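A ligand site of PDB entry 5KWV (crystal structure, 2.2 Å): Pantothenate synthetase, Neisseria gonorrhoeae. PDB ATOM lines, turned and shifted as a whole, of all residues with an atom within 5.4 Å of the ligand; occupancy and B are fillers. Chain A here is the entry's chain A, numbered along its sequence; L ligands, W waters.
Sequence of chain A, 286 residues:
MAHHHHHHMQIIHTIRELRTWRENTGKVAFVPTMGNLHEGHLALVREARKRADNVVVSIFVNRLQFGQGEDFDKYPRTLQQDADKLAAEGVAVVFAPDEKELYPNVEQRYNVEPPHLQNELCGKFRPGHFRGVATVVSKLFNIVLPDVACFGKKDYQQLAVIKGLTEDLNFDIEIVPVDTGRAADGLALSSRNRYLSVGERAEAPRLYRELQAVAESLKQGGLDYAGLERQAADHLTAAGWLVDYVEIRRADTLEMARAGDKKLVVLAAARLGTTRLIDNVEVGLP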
ATOM      1  N   PRO A  32       3.106 -30.507 -20.595  1.00  0.00           N
ATOM      2  CA  PRO A  32       4.113 -31.024 -19.653  1.00  0.00           C
ATOM      3  C   PRO A  32       3.637 -30.902 -18.213  1.00  0.00           C
ATOM      4  O   PRO A  32       3.099 -29.865 -17.808  1.00  0.00           O
ATOM      5  CB  PRO A  32       5.337 -30.150 -19.903  1.00  0.00           C
ATOM      6  CG  PRO A  32       4.788 -28.880 -20.487  1.00  0.00           C
ATOM      7  CD  PRO A  32       3.483 -29.195 -21.153  1.00  0.00           C
ATOM      8  N   THR A  33       3.835 -31.984 -17.443  1.00  0.00           N
ATOM      9  CA  THR A  33       3.406 -32.043 -16.055  1.00  0.00           C
ATOM     10  C   THR A  33       4.426 -32.795 -15.206  1.00  0.00           C
ATOM     11  O   THR A  33       5.314 -33.492 -15.719  1.00  0.00           O
ATOM     12  CB  THR A  33       2.052 -32.764 -15.836  1.00  0.00           C
ATOM     13  OG1 THR A  33       2.265 -34.180 -15.803  1.00  0.00           O
ATOM     14  CG2 THR A  33       1.045 -32.434 -16.919  1.00  0.00           C
ATOM     15  N   MET A  34       4.233 -32.697 -13.890  1.00  0.00           N
ATOM     16  CA  MET A  34       4.939 -33.504 -12.902  1.00  0.00           C
ATOM     17  C   MET A  34       4.070 -34.622 -12.344  1.00  0.00           C
ATOM     18  O   MET A  34       4.366 -35.145 -11.258  1.00  0.00           O
ATOM     19  CB  MET A  34       5.448 -32.642 -11.742  1.00  0.00           C
ATOM     20  CG  MET A  34       6.326 -31.449 -12.160  1.00  0.00           C
ATOM     21  SD  MET A  34       7.399 -30.846 -10.826  1.00  0.00           S
ATOM     22  CE  MET A  34       6.178 -30.307  -9.625  1.00  0.00           C
ATOM     23  N   GLY A  35       3.022 -35.030 -13.072  1.00  0.00           N
ATOM     24  CA  GLY A  35       2.198 -36.117 -12.579  1.00  0.00           C
ATOM     25  C   GLY A  35       1.291 -35.663 -11.423  1.00  0.00           C
ATOM     26  O   GLY A  35       1.053 -34.477 -11.214  1.00  0.00           O
ATOM     27  N   HIS A  38      -4.755 -33.889 -11.485  1.00  0.00           N
ATOM     28  CA  HIS A  38      -6.058 -33.530 -10.960  1.00  0.00           C
ATOM     29  C   HIS A  38      -6.797 -32.755 -12.041  1.00  0.00           C
ATOM     30  O   HIS A  38      -6.277 -32.542 -13.147  1.00  0.00           O
ATOM     31  CB  HIS A  38      -5.936 -32.715  -9.673  1.00  0.00           C
ATOM     32  CG  HIS A  38      -5.076 -31.509  -9.823  1.00  0.00           C
ATOM     33  ND1 HIS A  38      -5.419 -30.441 -10.629  1.00  0.00           N
ATOM     34  CD2 HIS A  38      -3.849 -31.215  -9.326  1.00  0.00           C
ATOM     35  CE1 HIS A  38      -4.464 -29.536 -10.616  1.00  0.00           C
ATOM     36  NE2 HIS A  38      -3.501 -29.982  -9.824  1.00  0.00           N
ATOM     37  N   GLY A  40      -7.431 -29.703 -12.559  1.00  0.00           N
ATOM     38  CA  GLY A  40      -6.715 -28.569 -13.133  1.00  0.00           C
ATOM     39  C   GLY A  40      -5.837 -28.939 -14.320  1.00  0.00           C
ATOM     40  O   GLY A  40      -5.777 -28.208 -15.318  1.00  0.00           O
ATOM     41  N   HIS A  41      -5.144 -30.098 -14.239  1.00  0.00           N
ATOM     42  CA  HIS A  41      -4.362 -30.588 -15.366  1.00  0.00           C
ATOM     43  C   HIS A  41      -5.257 -30.966 -16.540  1.00  0.00           C
ATOM     44  O   HIS A  41      -4.886 -30.771 -17.706  1.00  0.00           O
ATOM     45  CB  HIS A  41      -3.507 -31.794 -14.947  1.00  0.00           C
ATOM     46  CG  HIS A  41      -2.576 -31.520 -13.805  1.00  0.00           C
ATOM     47  ND1 HIS A  41      -2.765 -32.053 -12.548  1.00  0.00           N
ATOM     48  CD2 HIS A  41      -1.446 -30.779 -13.740  1.00  0.00           C
ATOM     49  CE1 HIS A  41      -1.784 -31.646 -11.752  1.00  0.00           C
ATOM     50  NE2 HIS A  41      -0.979 -30.867 -12.445  1.00  0.00           N
ATOM     51  N   ALA A  43      -7.958 -29.578 -17.436  1.00  0.00           N
ATOM     52  CA  ALA A  43      -8.268 -28.352 -18.175  1.00  0.00           C
ATOM     53  C   ALA A  43      -7.219 -28.102 -19.253  1.00  0.00           C
ATOM     54  O   ALA A  43      -7.563 -27.818 -20.405  1.00  0.00           O
ATOM     55  CB  ALA A  43      -8.367 -27.161 -17.227  1.00  0.00           C
ATOM     56  N   LEU A  44      -5.935 -28.232 -18.904  1.00  0.00           N
ATOM     57  CA  LEU A  44      -4.871 -28.103 -19.904  1.00  0.00           C
ATOM     58  C   LEU A  44      -5.047 -29.108 -21.027  1.00  0.00           C
ATOM     59  O   LEU A  44      -4.890 -28.776 -22.208  1.00  0.00           O
ATOM     60  CB  LEU A  44      -3.484 -28.297 -19.289  1.00  0.00           C
ATOM     61  CG  LEU A  44      -2.893 -27.419 -18.189  1.00  0.00           C
ATOM     62  CD1 LEU A  44      -1.376 -27.510 -18.215  1.00  0.00           C
ATOM     63  CD2 LEU A  44      -3.305 -25.993 -18.380  1.00  0.00           C
ATOM     64  N   CYS A 150       0.548 -26.136 -23.802  1.00  0.00           N
ATOM     65  CA  CYS A 150      -0.394 -25.533 -22.866  1.00  0.00           C
ATOM     66  C   CYS A 150       0.201 -25.444 -21.458  1.00  0.00           C
ATOM     67  O   CYS A 150       0.808 -26.399 -20.966  1.00  0.00           O
ATOM     68  CB  CYS A 150      -1.685 -26.346 -22.832  1.00  0.00           C
ATOM     69  SG  CYS A 150      -2.517 -26.448 -24.472  1.00  0.00           S
ATOM     70  N   PHE A 151       0.028 -24.290 -20.812  1.00  0.00           N
ATOM     71  CA  PHE A 151       0.504 -24.056 -19.464  1.00  0.00           C
ATOM     72  C   PHE A 151      -0.560 -23.313 -18.666  1.00  0.00           C
ATOM     73  O   PHE A 151      -1.379 -22.577 -19.234  1.00  0.00           O
ATOM     74  CB  PHE A 151       1.829 -23.273 -19.472  1.00  0.00           C
ATOM     75  CG  PHE A 151       2.926 -23.979 -20.198  1.00  0.00           C
ATOM     76  CD1 PHE A 151       3.797 -24.834 -19.523  1.00  0.00           C
ATOM     77  CD2 PHE A 151       3.086 -23.823 -21.573  1.00  0.00           C
ATOM     78  CE1 PHE A 151       4.809 -25.498 -20.198  1.00  0.00           C
ATOM     79  CE2 PHE A 151       4.111 -24.491 -22.254  1.00  0.00           C
ATOM     80  CZ  PHE A 151       4.976 -25.337 -21.559  1.00  0.00           C
ATOM     81  N   GLY A 152      -0.571 -23.542 -17.357  1.00  0.00           N
ATOM     82  CA  GLY A 152      -1.614 -22.995 -16.492  1.00  0.00           C
ATOM     83  C   GLY A 152      -1.266 -21.602 -15.989  1.00  0.00           C
ATOM     84  O   GLY A 152      -0.122 -21.316 -15.608  1.00  0.00           O
ATOM     85  N   LYS A 153      -2.281 -20.727 -15.968  1.00  0.00           N
ATOM     86  CA  LYS A 153      -2.102 -19.358 -15.512  1.00  0.00           C
ATOM     87  C   LYS A 153      -1.855 -19.281 -14.002  1.00  0.00           C
ATOM     88  O   LYS A 153      -1.354 -18.253 -13.533  1.00  0.00           O
ATOM     89  CB  LYS A 153      -3.330 -18.506 -15.868  1.00  0.00           C
ATOM     90  CG  LYS A 153      -3.335 -17.913 -17.267  1.00  0.00           C
ATOM     91  CD  LYS A 153      -4.708 -17.239 -17.511  1.00  0.00           C
ATOM     92  CE  LYS A 153      -4.628 -16.050 -18.445  1.00  0.00           C
ATOM     93  NZ  LYS A 153      -5.978 -15.371 -18.600  1.00  0.00           N
ATOM     94  N   LYS A 154      -2.222 -20.313 -13.249  1.00  0.00           N
ATOM     95  CA  LYS A 154      -1.930 -20.321 -11.822  1.00  0.00           C
ATOM     96  C   LYS A 154      -0.430 -20.125 -11.589  1.00  0.00           C
ATOM     97  O   LYS A 154      -0.011 -19.427 -10.665  1.00  0.00           O
ATOM     98  CB  LYS A 154      -2.406 -21.632 -11.199  1.00  0.00           C
ATOM     99  CG  LYS A 154      -2.157 -21.761  -9.698  1.00  0.00           C
ATOM    100  CD  LYS A 154      -2.281 -23.216  -9.216  1.00  0.00           C
ATOM    101  CE  LYS A 154      -0.936 -23.927  -9.297  1.00  0.00           C
ATOM    102  NZ  LYS A 154      -1.007 -25.394  -9.000  1.00  0.00           N
ATOM    103  N   ASP A 155       0.389 -20.733 -12.439  1.00  0.00           N
ATOM    104  CA  ASP A 155       1.842 -20.534 -12.338  1.00  0.00           C
ATOM    105  C   ASP A 155       2.241 -19.429 -13.326  1.00  0.00           C
ATOM    106  O   ASP A 155       2.839 -19.651 -14.372  1.00  0.00           O
ATOM    107  CB  ASP A 155       2.567 -21.824 -12.601  1.00  0.00           C
ATOM    108  CG  ASP A 155       2.163 -22.902 -11.625  1.00  0.00           C
ATOM    109  OD1 ASP A 155       2.719 -22.933 -10.495  1.00  0.00           O
ATOM    110  OD2 ASP A 155       1.271 -23.690 -11.978  1.00  0.00           O
ATOM    111  N   GLN A 158       5.994 -18.824 -14.111  1.00  0.00           N
ATOM    112  CA  GLN A 158       6.411 -19.894 -15.005  1.00  0.00           C
ATOM    113  C   GLN A 158       5.945 -19.656 -16.437  1.00  0.00           C
ATOM    114  O   GLN A 158       6.713 -19.808 -17.389  1.00  0.00           O
ATOM    115  CB  GLN A 158       5.859 -21.200 -14.473  1.00  0.00           C
ATOM    116  CG  GLN A 158       5.944 -22.364 -15.415  1.00  0.00           C
ATOM    117  CD  GLN A 158       5.492 -23.626 -14.713  1.00  0.00           C
ATOM    118  OE1 GLN A 158       6.249 -24.220 -13.935  1.00  0.00           O
ATOM    119  NE2 GLN A 158       4.222 -24.016 -14.947  1.00  0.00           N
ATOM    120  N   VAL A 178      -3.826 -21.406 -20.021  1.00  0.00           N
ATOM    121  CA  VAL A 178      -5.128 -21.956 -19.627  1.00  0.00           C
ATOM    122  C   VAL A 178      -5.503 -21.445 -18.243  1.00  0.00           C
ATOM    123  O   VAL A 178      -4.672 -21.436 -17.314  1.00  0.00           O
ATOM    124  CB  VAL A 178      -5.115 -23.487 -19.670  1.00  0.00           C
ATOM    125  CG1 VAL A 178      -6.478 -24.054 -19.293  1.00  0.00           C
ATOM    126  CG2 VAL A 178      -4.709 -23.978 -21.050  1.00  0.00           C
ATOM    127  N   ASP A 179      -6.760 -21.065 -18.093  1.00  0.00           N
ATOM    128  CA  ASP A 179      -7.222 -20.433 -16.865  1.00  0.00           C
ATOM    129  C   ASP A 179      -7.168 -21.436 -15.716  1.00  0.00           C
ATOM    130  O   ASP A 179      -7.346 -22.647 -15.900  1.00  0.00           O
ATOM    131  CB  ASP A 179      -8.653 -19.894 -17.043  1.00  0.00           C
ATOM    132  CG  ASP A 179      -8.687 -18.533 -17.724  1.00  0.00           C
ATOM    133  OD1 ASP A 179      -7.901 -17.636 -17.338  1.00  0.00           O
ATOM    134  OD2 ASP A 179      -9.479 -18.386 -18.682  1.00  0.00           O
ATOM    135  N   THR A 180      -6.939 -20.903 -14.514  1.00  0.00           N
ATOM    136  CA  THR A 180      -6.829 -21.719 -13.319  1.00  0.00           C
ATOM    137  C   THR A 180      -8.155 -22.400 -12.986  1.00  0.00           C
ATOM    138  O   THR A 180      -9.175 -21.725 -12.789  1.00  0.00           O
ATOM    139  CB  THR A 180      -6.371 -20.829 -12.148  1.00  0.00           C
ATOM    140  OG1 THR A 180      -5.105 -20.247 -12.480  1.00  0.00           O
ATOM    141  CG2 THR A 180      -6.277 -21.626 -10.816  1.00  0.00           C
ATOM    142  N   GLY A 181      -8.156 -23.727 -12.993  1.00  0.00           N
ATOM    143  CA  GLY A 181      -9.280 -24.468 -12.425  1.00  0.00           C
ATOM    144  C   GLY A 181      -9.269 -24.358 -10.913  1.00  0.00           C
ATOM    145  O   GLY A 181      -8.233 -24.474 -10.259  1.00  0.00           O
ATOM    146  N   ARG A 182     -10.455 -24.163 -10.341  1.00  0.00           N
ATOM    147  CA  ARG A 182     -10.632 -23.908  -8.921  1.00  0.00           C
ATOM    148  C   ARG A 182     -11.611 -24.882  -8.285  1.00  0.00           C
ATOM    149  O   ARG A 182     -12.498 -25.442  -8.946  1.00  0.00           O
ATOM    150  CB  ARG A 182     -11.138 -22.467  -8.670  1.00  0.00           C
ATOM    151  CG  ARG A 182     -10.145 -21.396  -9.129  1.00  0.00           C
ATOM    152  CD  ARG A 182     -10.626 -19.948  -8.955  1.00  0.00           C
ATOM    153  NE  ARG A 182      -9.588 -19.083  -9.491  1.00  0.00           N
ATOM    154  CZ  ARG A 182      -8.438 -18.832  -8.866  1.00  0.00           C
ATOM    155  NH1 ARG A 182      -8.214 -19.344  -7.659  1.00  0.00           N
ATOM    156  NH2 ARG A 182      -7.515 -18.069  -9.438  1.00  0.00           N
ATOM    157  N   ALA A 188      -7.499 -22.564  -5.677  1.00  0.00           N
ATOM    158  CA  ALA A 188      -6.872 -23.041  -6.897  1.00  0.00           C
ATOM    159  C   ALA A 188      -6.414 -24.491  -6.729  1.00  0.00           C
ATOM    160  O   ALA A 188      -5.671 -24.810  -5.791  1.00  0.00           O
ATOM    161  CB  ALA A 188      -5.688 -22.150  -7.254  1.00  0.00           C
ATOM    162  N   LEU A 189      -6.849 -25.360  -7.635  1.00  0.00           N
ATOM    163  CA  LEU A 189      -6.502 -26.767  -7.572  1.00  0.00           C
ATOM    164  C   LEU A 189      -4.992 -26.960  -7.717  1.00  0.00           C
ATOM    165  O   LEU A 189      -4.343 -26.320  -8.555  1.00  0.00           O
ATOM    166  CB  LEU A 189      -7.255 -27.558  -8.645  1.00  0.00           C
ATOM    167  CG  LEU A 189      -8.779 -27.505  -8.535  1.00  0.00           C
ATOM    168  CD1 LEU A 189      -9.509 -28.271  -9.661  1.00  0.00           C
ATOM    169  CD2 LEU A 189      -9.191 -28.095  -7.187  1.00  0.00           C
ATOM    170  N   SER A 190      -4.440 -27.856  -6.905  1.00  0.00           N
ATOM    171  CA  SER A 190      -3.010 -28.119  -6.892  1.00  0.00           C
ATOM    172  C   SER A 190      -2.742 -29.433  -6.177  1.00  0.00           C
ATOM    173  O   SER A 190      -3.484 -29.825  -5.271  1.00  0.00           O
ATOM    174  CB  SER A 190      -2.259 -26.969  -6.212  1.00  0.00           C
ATOM    175  OG  SER A 190      -0.882 -27.260  -6.081  1.00  0.00           O
ATOM    176  N   SER A 191      -1.695 -30.138  -6.627  1.00  0.00           N
ATOM    177  CA  SER A 191      -1.281 -31.365  -5.962  1.00  0.00           C
ATOM    178  C   SER A 191      -0.963 -31.121  -4.488  1.00  0.00           C
ATOM    179  O   SER A 191      -1.234 -31.959  -3.638  1.00  0.00           O
ATOM    180  CB  SER A 191      -0.057 -31.960  -6.667  1.00  0.00           C
ATOM    181  OG  SER A 191      -0.296 -32.177  -8.047  1.00  0.00           O
ATOM    182  N   ARG A 192      -0.413 -29.935  -4.176  1.00  0.00           N
ATOM    183  CA  ARG A 192      -0.065 -29.571  -2.805  1.00  0.00           C
ATOM    184  C   ARG A 192      -1.264 -29.569  -1.873  1.00  0.00           C
ATOM    185  O   ARG A 192      -1.077 -29.667  -0.653  1.00  0.00           O
ATOM    186  CB  ARG A 192       0.622 -28.205  -2.797  1.00  0.00           C
HETATM  187  P1  LIG L   1       2.672 -28.870  -7.449  1.00  0.00           P
HETATM  188  O1  LIG L   1       3.980 -29.654  -7.041  1.00  0.00           O
HETATM  189  O2  LIG L   1       1.708 -28.895  -6.298  1.00  0.00           O
HETATM  190  O3  LIG L   1       3.048 -27.373  -7.811  1.00  0.00           O
HETATM  191  P2  LIG L   1       1.061 -28.672  -9.780  1.00  0.00           P
HETATM  192  O4  LIG L   1       1.580 -27.197  -9.790  1.00  0.00           O
HETATM  193  O5  LIG L   1      -0.372 -28.716  -9.335  1.00  0.00           O
HETATM  194  N1  LIG L   1       2.009 -29.655  -8.799  1.00  0.00           N
HETATM  195  P3  LIG L   1       2.402 -29.138 -12.114  1.00  0.00           P
HETATM  196  O6  LIG L   1       3.466 -28.456 -11.266  1.00  0.00           O
HETATM  197  O7  LIG L   1       2.759 -30.477 -12.673  1.00  0.00           O
HETATM  198  O8  LIG L   1       1.109 -29.245 -11.220  1.00  0.00           O
HETATM  199  O9  LIG L   1       1.882 -28.242 -13.320  1.00  0.00           O
HETATM  200  C1  LIG L   1       1.723 -28.809 -14.635  1.00  0.00           C
HETATM  201  C2  LIG L   1       0.924 -27.835 -15.480  1.00  0.00           C
HETATM  202  O10 LIG L   1      -0.431 -27.767 -14.982  1.00  0.00           O
HETATM  203  C3  LIG L   1       1.470 -26.399 -15.457  1.00  0.00           C
HETATM  204  O11 LIG L   1       1.385 -25.790 -16.738  1.00  0.00           O
HETATM  205  C4  LIG L   1       0.563 -25.732 -14.424  1.00  0.00           C
HETATM  206  O12 LIG L   1       0.462 -24.316 -14.549  1.00  0.00           O
HETATM  207  C5  LIG L   1      -0.771 -26.422 -14.725  1.00  0.00           C
HETATM  208  N2  LIG L   1      -1.721 -26.343 -13.628  1.00  0.00           N
HETATM  209  C6  LIG L   1      -1.532 -26.733 -12.322  1.00  0.00           C
HETATM  210  N3  LIG L   1      -2.552 -26.493 -11.538  1.00  0.00           N
HETATM  211  C7  LIG L   1      -3.477 -25.878 -12.371  1.00  0.00           C
HETATM  212  C8  LIG L   1      -4.773 -25.367 -12.156  1.00  0.00           C
HETATM  213  N4  LIG L   1      -5.389 -25.400 -10.965  1.00  0.00           N
HETATM  214  N5  LIG L   1      -5.420 -24.819 -13.205  1.00  0.00           N
HETATM  215  C9  LIG L   1      -4.804 -24.786 -14.396  1.00  0.00           C
HETATM  216  N6  LIG L   1      -3.597 -25.230 -14.716  1.00  0.00           N
HETATM  217  C10 LIG L   1      -2.976 -25.771 -13.656  1.00  0.00           C
HETATM  218  O   HOH W   1       2.415 -22.199 -16.035  1.00  0.00           O
HETATM  219  O   HOH W   2       5.653 -26.016  -9.372  1.00  0.00           O
HETATM  220  O   HOH W   3       2.029 -27.521 -18.628  1.00  0.00           O
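N of Ser 191 is in hydrogen-bond range of O5 of the ligand.
OD2 of Asp 155 lies within hydrogen-bond range of O12 of the ligand (2.8 Å).
O11 of the ligand lies within hydrogen-bond range of N of Gly 152.
OG of Ser 191 lies within hydrogen-bond range of N1 of the ligand (3.5 Å).
N4 of the ligand lies within hydrogen-bond range of O of Gly 181 (3.1 Å).
NZ of Lys 154 is in salt-bridge range of O4 of the ligand (3.3 Å).
A nitrogen (N4) of the ligand is in hydrogen-bond range of the backbone carbonyl oxygen of Leu 189, at 2.8 Å.
The backbone NH (N) of Met 34 sits at hydrogen-bond distance from an oxygen (O7) of the ligand (2.9 Å).
O2 of the ligand sits at hydrogen-bond distance from N of Arg 192 (3.2 Å).
A ring nitrogen (NE2) of His 41 lies within hydrogen-bond range of an oxygen (O8) of the ligand (2.9 Å).
An oxygen (O12) of the ligand sits close to the backbone carbonyl oxygen (O) of Gly 152 (3.2 Å).
A nitrogen (N5) of the ligand is in hydrogen-bond range of the backbone NH of Gly 181.
O5 of the ligand lies within hydrogen-bond range of NE2 of His 38.
OG of Ser 190 is in hydrogen-bond range of O2 of the ligand, at 3.1 Å.
N of Leu 189 is in hydrogen-bond range of O of Gly 181 (3.1 Å).
The side-chain carboxylate (OD1) of Asp 179 is in salt-bridge range of the side-chain amino group (NZ) of Lys 153.
The side-chain hydroxyl of Thr 33 lies within hydrogen-bond range of the backbone NH of Gly 35 (3.0 Å).
OG of Ser 190 sits close to N of Arg 192, at 3.3 Å.
The side-chain amino group (NZ) of Lys 154 lies within hydrogen-bond range of the backbone carbonyl oxygen (O) of Leu 189.
The backbone NH of Val 178 is in hydrogen-bond range of the backbone carbonyl oxygen of Phe 151, 2.8 Å away.
The side-chain amino group of Lys 154 lies close to the side-chain hydroxyl of Ser 190 (3.5 Å).
N of Lys 154 is in hydrogen-bond range of OG1 of Thr 180, 3.0 Å away.
Water W3 lies within hydrogen-bond range of an oxygen (O11) of the ligand (2.6 Å), the backbone carbonyl oxygen (O) of Pro 32 (2.7 Å) and the backbone carbonyl oxygen (O) of Cys 150 (2.9 Å).
Water W1 lies within hydrogen-bond range of O of Gly 152 (2.7 Å), NE2 of Gln 158 (2.8 Å), O of Asp 155 (3.1 Å) and O12 of the ligand (3.2 Å).
Pro 32 touches the ligand.
Thr 33 touches the ligand (CA to O7, 3.8 Å).
Gly 40 touches the ligand.
Leu 44 touches the ligand.
CA of Phe 151 touches O11 of the ligand (3.3 Å).
Gln 158 touches the ligand (NE2 to C3, 3.7 Å).
O of Asp 179 touches C9 of the ligand, 3.6 Å away.
Thr 180 touches the ligand (CA to N5, 3.4 Å).
19 residues have an atom within 4 Å of the ligand: Pro 32, Thr 33, Met 34, His 38, Gly 40, His 41, Leu 44, Phe 151, Gly 152, Lys 154, Asp 155, Gln 158, Asp 179, Thr 180, Gly 181, Leu 189, Ser 190, Ser 191 and Arg 192.
Along chain A the residues within 4 Å of the ligand span positions 32 to 192.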
